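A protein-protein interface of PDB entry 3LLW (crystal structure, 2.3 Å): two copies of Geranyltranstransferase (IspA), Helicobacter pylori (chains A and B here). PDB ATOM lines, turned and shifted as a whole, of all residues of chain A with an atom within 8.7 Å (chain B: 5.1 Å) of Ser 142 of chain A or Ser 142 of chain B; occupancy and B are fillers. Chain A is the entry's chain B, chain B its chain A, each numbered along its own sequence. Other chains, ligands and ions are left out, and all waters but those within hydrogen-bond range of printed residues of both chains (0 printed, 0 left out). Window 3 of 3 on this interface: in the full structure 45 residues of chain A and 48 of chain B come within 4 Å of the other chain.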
ATOM      1  N   LEU A 135      24.053  12.517 -16.457  1.00  0.00           N
ATOM      2  CA  LEU A 135      23.387  11.683 -17.442  1.00  0.00           C
ATOM      3  C   LEU A 135      21.878  11.920 -17.406  1.00  0.00           C
ATOM      4  O   LEU A 135      21.256  12.093 -18.449  1.00  0.00           O
ATOM      5  CB  LEU A 135      23.695  10.221 -17.168  1.00  0.00           C
ATOM      6  CG  LEU A 135      23.969   9.253 -18.307  1.00  0.00           C
ATOM      7  CD1 LEU A 135      24.853   9.888 -19.318  1.00  0.00           C
ATOM      8  CD2 LEU A 135      24.637   8.019 -17.738  1.00  0.00           C
ATOM      9  N   SER A 136      21.310  11.970 -16.198  1.00  0.00           N
ATOM     10  CA  SER A 136      19.871  12.089 -16.033  1.00  0.00           C
ATOM     11  C   SER A 136      19.351  13.480 -16.369  1.00  0.00           C
ATOM     12  O   SER A 136      18.172  13.637 -16.624  1.00  0.00           O
ATOM     13  CB  SER A 136      19.435  11.694 -14.621  1.00  0.00           C
ATOM     14  OG  SER A 136      19.820  12.666 -13.662  1.00  0.00           O
ATOM     15  N   ALA A 138      20.634  15.309 -19.024  1.00  0.00           N
ATOM     16  CA  ALA A 138      20.815  15.516 -20.475  1.00  0.00           C
ATOM     17  C   ALA A 138      19.481  15.425 -21.218  1.00  0.00           C
ATOM     18  O   ALA A 138      18.726  14.476 -21.018  1.00  0.00           O
ATOM     19  CB  ALA A 138      21.790  14.494 -21.047  1.00  0.00           C
ATOM     20  N   LEU A 139      19.206  16.390 -22.093  1.00  0.00           N
ATOM     21  CA  LEU A 139      17.856  16.530 -22.683  1.00  0.00           C
ATOM     22  C   LEU A 139      17.631  15.733 -23.963  1.00  0.00           C
ATOM     23  O   LEU A 139      17.358  16.290 -25.020  1.00  0.00           O
ATOM     24  CB  LEU A 139      17.470  18.003 -22.872  1.00  0.00           C
ATOM     25  CG  LEU A 139      17.360  18.889 -21.625  1.00  0.00           C
ATOM     26  CD1 LEU A 139      17.378  20.365 -22.004  1.00  0.00           C
ATOM     27  CD2 LEU A 139      16.120  18.556 -20.804  1.00  0.00           C
ATOM     28  N   LEU A 140      17.760  14.419 -23.850  1.00  0.00           N
ATOM     29  CA  LEU A 140      17.404  13.500 -24.914  1.00  0.00           C
ATOM     30  C   LEU A 140      16.144  12.794 -24.467  1.00  0.00           C
ATOM     31  O   LEU A 140      15.673  13.019 -23.352  1.00  0.00           O
ATOM     32  CB  LEU A 140      18.518  12.483 -25.165  1.00  0.00           C
ATOM     33  CG  LEU A 140      19.941  12.978 -25.424  1.00  0.00           C
ATOM     34  CD1 LEU A 140      20.796  11.773 -25.706  1.00  0.00           C
ATOM     35  CD2 LEU A 140      20.036  13.996 -26.579  1.00  0.00           C
ATOM     36  N   GLU A 141      15.591  11.954 -25.337  1.00  0.00           N
ATOM     37  CA  GLU A 141      14.383  11.214 -25.021  1.00  0.00           C
ATOM     38  C   GLU A 141      14.632  10.298 -23.847  1.00  0.00           C
ATOM     39  O   GLU A 141      15.727   9.726 -23.706  1.00  0.00           O
ATOM     40  CB  GLU A 141      13.890  10.442 -26.240  1.00  0.00           C
ATOM     41  CG  GLU A 141      13.051  11.318 -27.173  1.00  0.00           C
ATOM     42  CD  GLU A 141      12.902  10.760 -28.580  1.00  0.00           C
ATOM     43  OE1 GLU A 141      13.313   9.601 -28.836  1.00  0.00           O
ATOM     44  OE2 GLU A 141      12.365  11.496 -29.437  1.00  0.00           O
ATOM     45  N   SER A 142      13.622  10.183 -22.992  1.00  0.00           N
ATOM     46  CA  SER A 142      13.790   9.585 -21.681  1.00  0.00           C
ATOM     47  C   SER A 142      14.214   8.123 -21.786  1.00  0.00           C
ATOM     48  O   SER A 142      15.020   7.649 -20.976  1.00  0.00           O
ATOM     49  CB  SER A 142      12.508   9.736 -20.874  1.00  0.00           C
ATOM     50  OG  SER A 142      11.441   9.144 -21.584  1.00  0.00           O
ATOM     51  N   HIS A 143      13.705   7.434 -22.810  1.00  0.00           N
ATOM     52  CA  HIS A 143      14.089   6.062 -23.082  1.00  0.00           C
ATOM     53  C   HIS A 143      15.570   5.930 -23.449  1.00  0.00           C
ATOM     54  O   HIS A 143      16.198   4.935 -23.081  1.00  0.00           O
ATOM     55  CB  HIS A 143      13.159   5.385 -24.113  1.00  0.00           C
ATOM     56  CG  HIS A 143      13.395   5.803 -25.536  1.00  0.00           C
ATOM     57  ND1 HIS A 143      14.083   5.020 -26.438  1.00  0.00           N
ATOM     58  CD2 HIS A 143      13.014   6.910 -26.217  1.00  0.00           C
ATOM     59  CE1 HIS A 143      14.123   5.629 -27.610  1.00  0.00           C
ATOM     60  NE2 HIS A 143      13.484   6.779 -27.503  1.00  0.00           N
ATOM     61  N   ILE A 144      16.123   6.934 -24.140  1.00  0.00           N
ATOM     62  CA  ILE A 144      17.557   6.964 -24.469  1.00  0.00           C
ATOM     63  C   ILE A 144      18.380   7.115 -23.178  1.00  0.00           C
ATOM     64  O   ILE A 144      19.297   6.337 -22.938  1.00  0.00           O
ATOM     65  CB  ILE A 144      17.916   8.133 -25.439  1.00  0.00           C
ATOM     66  CG1 ILE A 144      17.047   8.120 -26.712  1.00  0.00           C
ATOM     67  CG2 ILE A 144      19.419   8.162 -25.742  1.00  0.00           C
ATOM     68  CD1 ILE A 144      17.441   7.111 -27.760  1.00  0.00           C
ATOM     69  N   ILE A 145      18.013   8.099 -22.352  1.00  0.00           N
ATOM     70  CA  ILE A 145      18.677   8.389 -21.083  1.00  0.00           C
ATOM     71  C   ILE A 145      18.731   7.145 -20.185  1.00  0.00           C
ATOM     72  O   ILE A 145      19.798   6.775 -19.720  1.00  0.00           O
ATOM     73  CB  ILE A 145      18.017   9.591 -20.339  1.00  0.00           C
ATOM     74  CG1 ILE A 145      18.048  10.863 -21.192  1.00  0.00           C
ATOM     75  CG2 ILE A 145      18.685   9.836 -18.971  1.00  0.00           C
ATOM     76  CD1 ILE A 145      19.453  11.261 -21.713  1.00  0.00           C
ATOM     77  N   VAL A 146      17.581   6.496 -19.997  1.00  0.00           N
ATOM     78  CA  VAL A 146      17.454   5.288 -19.179  1.00  0.00           C
ATOM     79  C   VAL A 146      18.439   4.186 -19.600  1.00  0.00           C
ATOM     80  O   VAL A 146      19.173   3.652 -18.749  1.00  0.00           O
ATOM     81  CB  VAL A 146      15.971   4.800 -19.119  1.00  0.00           C
ATOM     82  CG1 VAL A 146      15.868   3.381 -18.644  1.00  0.00           C
ATOM     83  CG2 VAL A 146      15.151   5.713 -18.211  1.00  0.00           C
ATOM     84  N   GLU A 147      18.490   3.895 -20.905  1.00  0.00           N
ATOM     85  CA  GLU A 147      19.422   2.906 -21.466  1.00  0.00           C
ATOM     86  C   GLU A 147      20.892   3.245 -21.238  1.00  0.00           C
ATOM     87  O   GLU A 147      21.678   2.352 -20.933  1.00  0.00           O
ATOM     88  CB  GLU A 147      19.179   2.664 -22.965  1.00  0.00           C
ATOM     89  CG  GLU A 147      17.841   2.015 -23.320  1.00  0.00           C
ATOM     90  CD  GLU A 147      17.633   0.641 -22.673  1.00  0.00           C
ATOM     91  OE1 GLU A 147      16.609   0.456 -21.975  1.00  0.00           O
ATOM     92  OE2 GLU A 147      18.493  -0.249 -22.860  1.00  0.00           O
ATOM     93  N   LEU A 148      21.264   4.520 -21.367  1.00  0.00           N
ATOM     94  CA  LEU A 148      22.650   4.942 -21.064  1.00  0.00           C
ATOM     95  C   LEU A 148      23.032   4.713 -19.613  1.00  0.00           C
ATOM     96  O   LEU A 148      24.186   4.333 -19.320  1.00  0.00           O
ATOM     97  CB  LEU A 148      22.891   6.402 -21.410  1.00  0.00           C
ATOM     98  CG  LEU A 148      22.597   6.859 -22.844  1.00  0.00           C
ATOM     99  CD1 LEU A 148      22.492   8.349 -22.871  1.00  0.00           C
ATOM    100  CD2 LEU A 148      23.676   6.385 -23.792  1.00  0.00           C
ATOM    101  N   ILE A 149      22.066   4.939 -18.714  1.00  0.00           N
ATOM    102  CA  ILE A 149      22.285   4.745 -17.275  1.00  0.00           C
ATOM    103  C   ILE A 149      22.454   3.267 -16.958  1.00  0.00           C
ATOM    104  O   ILE A 149      23.359   2.901 -16.200  1.00  0.00           O
ATOM    105  CB  ILE A 149      21.213   5.454 -16.409  1.00  0.00           C
ATOM    106  CG1 ILE A 149      21.231   6.960 -16.731  1.00  0.00           C
ATOM    107  CG2 ILE A 149      21.465   5.234 -14.920  1.00  0.00           C
ATOM    108  CD1 ILE A 149      20.162   7.806 -16.089  1.00  0.00           C
ATOM    109  N   VAL A 202      23.768   4.132 -28.592  1.00  0.00           N
ATOM    110  CA  VAL A 202      22.480   4.366 -27.926  1.00  0.00           C
ATOM    111  C   VAL A 202      22.067   5.837 -27.978  1.00  0.00           C
ATOM    112  O   VAL A 202      20.922   6.150 -28.336  1.00  0.00           O
ATOM    113  CB  VAL A 202      22.480   3.792 -26.482  1.00  0.00           C
ATOM    114  CG1 VAL A 202      21.257   4.268 -25.653  1.00  0.00           C
ATOM    115  CG2 VAL A 202      22.516   2.270 -26.548  1.00  0.00           C
ATOM    116  N   LEU B 140       9.115   1.072 -14.880  1.00  0.00           N
ATOM    117  CA  LEU B 140       8.064   2.085 -14.945  1.00  0.00           C
ATOM    118  C   LEU B 140       8.320   2.918 -16.197  1.00  0.00           C
ATOM    119  O   LEU B 140       9.254   2.632 -16.943  1.00  0.00           O
ATOM    120  CB  LEU B 140       8.038   2.966 -13.687  1.00  0.00           C
ATOM    121  CG  LEU B 140       8.129   2.367 -12.271  1.00  0.00           C
ATOM    122  CD1 LEU B 140       7.912   3.454 -11.215  1.00  0.00           C
ATOM    123  CD2 LEU B 140       7.147   1.207 -12.039  1.00  0.00           C
ATOM    124  N   GLU B 141       7.491   3.935 -16.433  1.00  0.00           N
ATOM    125  CA  GLU B 141       7.618   4.782 -17.619  1.00  0.00           C
ATOM    126  C   GLU B 141       8.941   5.502 -17.587  1.00  0.00           C
ATOM    127  O   GLU B 141       9.376   5.952 -16.527  1.00  0.00           O
ATOM    128  CB  GLU B 141       6.479   5.794 -17.704  1.00  0.00           C
ATOM    129  CG  GLU B 141       5.166   5.211 -18.203  1.00  0.00           C
ATOM    130  CD  GLU B 141       3.992   6.143 -17.957  1.00  0.00           C
ATOM    131  OE1 GLU B 141       3.512   6.219 -16.800  1.00  0.00           O
ATOM    132  OE2 GLU B 141       3.547   6.801 -18.926  1.00  0.00           O
ATOM    133  N   SER B 142       9.578   5.597 -18.752  1.00  0.00           N
ATOM    134  CA  SER B 142      10.931   6.112 -18.856  1.00  0.00           C
ATOM    135  C   SER B 142      11.101   7.475 -18.199  1.00  0.00           C
ATOM    136  O   SER B 142      12.084   7.693 -17.476  1.00  0.00           O
ATOM    137  CB  SER B 142      11.431   6.092 -20.306  1.00  0.00           C
ATOM    138  OG  SER B 142      10.622   6.888 -21.148  1.00  0.00           O
ATOM    139  N   HIS B 143      10.126   8.361 -18.388  1.00  0.00           N
ATOM    140  CA  HIS B 143      10.200   9.698 -17.808  1.00  0.00           C
ATOM    141  C   HIS B 143      10.147   9.688 -16.278  1.00  0.00           C
ATOM    142  O   HIS B 143      10.732  10.562 -15.640  1.00  0.00           O
ATOM    143  CB  HIS B 143       9.153  10.648 -18.410  1.00  0.00           C
ATOM    144  CG  HIS B 143       7.751  10.372 -17.970  1.00  0.00           C
ATOM    145  ND1 HIS B 143       6.943   9.446 -18.596  1.00  0.00           N
ATOM    146  CD2 HIS B 143       7.006  10.911 -16.974  1.00  0.00           C
ATOM    147  CE1 HIS B 143       5.765   9.421 -17.997  1.00  0.00           C
ATOM    148  NE2 HIS B 143       5.776  10.302 -17.011  1.00  0.00           N
ATOM    149  N   ILE B 144       9.470   8.691 -15.702  1.00  0.00           N
ATOM    150  CA  ILE B 144       9.430   8.537 -14.250  1.00  0.00           C
ATOM    151  C   ILE B 144      10.789   8.070 -13.712  1.00  0.00           C
ATOM    152  O   ILE B 144      11.277   8.620 -12.718  1.00  0.00           O
ATOM    153  CB  ILE B 144       8.256   7.616 -13.781  1.00  0.00           C
ATOM    154  CG1 ILE B 144       6.905   8.332 -13.962  1.00  0.00           C
ATOM    155  CG2 ILE B 144       8.446   7.148 -12.312  1.00  0.00           C
ATOM    156  CD1 ILE B 144       5.679   7.421 -13.802  1.00  0.00           C
ATOM    157  N   ILE B 145      11.411   7.099 -14.389  1.00  0.00           N
ATOM    158  CA  ILE B 145      12.748   6.608 -13.992  1.00  0.00           C
ATOM    159  C   ILE B 145      13.806   7.723 -14.058  1.00  0.00           C
ATOM    160  O   ILE B 145      14.659   7.836 -13.159  1.00  0.00           O
ATOM    161  CB  ILE B 145      13.194   5.350 -14.806  1.00  0.00           C
ATOM    162  CG1 ILE B 145      12.165   4.220 -14.683  1.00  0.00           C
ATOM    163  CG2 ILE B 145      14.560   4.836 -14.354  1.00  0.00           C
ATOM    164  CD1 ILE B 145      11.728   3.902 -13.262  1.00  0.00           C
ATOM    165  N   VAL B 146      13.719   8.567 -15.088  1.00  0.00           N
ATOM    166  CA  VAL B 146      14.645   9.690 -15.235  1.00  0.00           C
ATOM    167  C   VAL B 146      14.533  10.667 -14.070  1.00  0.00           C
ATOM    168  O   VAL B 146      15.548  10.964 -13.424  1.00  0.00           O
ATOM    169  CB  VAL B 146      14.529  10.390 -16.602  1.00  0.00           C
ATOM    170  CG1 VAL B 146      15.181  11.774 -16.577  1.00  0.00           C
ATOM    171  CG2 VAL B 146      15.196   9.531 -17.656  1.00  0.00           C
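OG of Ser 142 of chain A lies within hydrogen-bond range of OG of Ser 142 of chain B (2.4 Å).
OE1 of Glu 141 of chain A is in hydrogen-bond range of NE2 of His 143 of chain A, 3.1 Å away.
Among the printed residues, pairs that only touch across the chains: Ser 136 of chain A with Val 146 of chain B, Ser 142 of chain A with His 143 of chain B, Ser 142 of chain A with Val 146 of chain B, His 143 of chain A with Ser 142 of chain B, Ile 145 of chain A with Val 146 of chain B, Val 146 of chain A with Ser 142 of chain B, Val 146 of chain A with Ile 145 of chain B and Val 146 of chain A with Val 146 of chain B.
Leu 135 of chain A touches none of the printed residues of chain B.
Of chain B, only Ser 142 (2.4 Å), His 143 (3.5 Å) and Val 146 (3.8 Å) come within 4 Å of Ser 142 of chain A.
Printed residues of chain B within 4 Å of Val 146 of chain A: Ser 142 (3.7 Å), Ile 145 (3.9 Å) and Val 146 (3.9 Å).
Leu 140 of chain B touches none of the printed residues of chain A.
Of chain A, only Ser 142 (2.4 Å), His 143 (3.5 Å) and Val 146 (3.7 Å) come within 4 Å of Ser 142 of chain B.
Of the printed residues of chain A, His 143 of chain B touches Ser 142.
Printed residues of chain A within 4 Å of Val 146 of chain B: Ser 136, Ser 142, Ile 145 and Val 146.
Hydrophobic or aromatic side chains of chain B within 4 Å of the printed part of chain A: Ile 145 and Val 146.
Along chain B the printed residues that touch a printed residue of chain A span positions 142 to 146.
Of the 15 printed residues of chain A, 5 touch a printed residue of chain B.
Hydrophobic or aromatic side chains of chain A within 4 Å of the printed part of chain B: Ile 145 and Val 146.
Among the printed residues, no Asp or Glu carboxylate lies within 4 Å of a Lys or Arg side-chain nitrogen of the other chain.
Ser 142 of chain B touches its own counterpart, Ser 142 of chain A.
Ser 142 of chain A touches His 143 of chain B, and with the chains exchanged His 143 of chain A touches Ser 142 of chain B.
Ser 142 of chain A touches Val 146 of chain B, and with the chains exchanged Val 146 of chain A touches Ser 142 of chain B.
Ile 145 of chain A touches Val 146 of chain B, and with the chains exchanged Val 146 of chain A touches Ile 145 of chain B.
7 positions are printed for both chains.
Of the 9 pairs that touch across the chains among the printed residues, 8 have their exchanged pair printed and touching as well.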
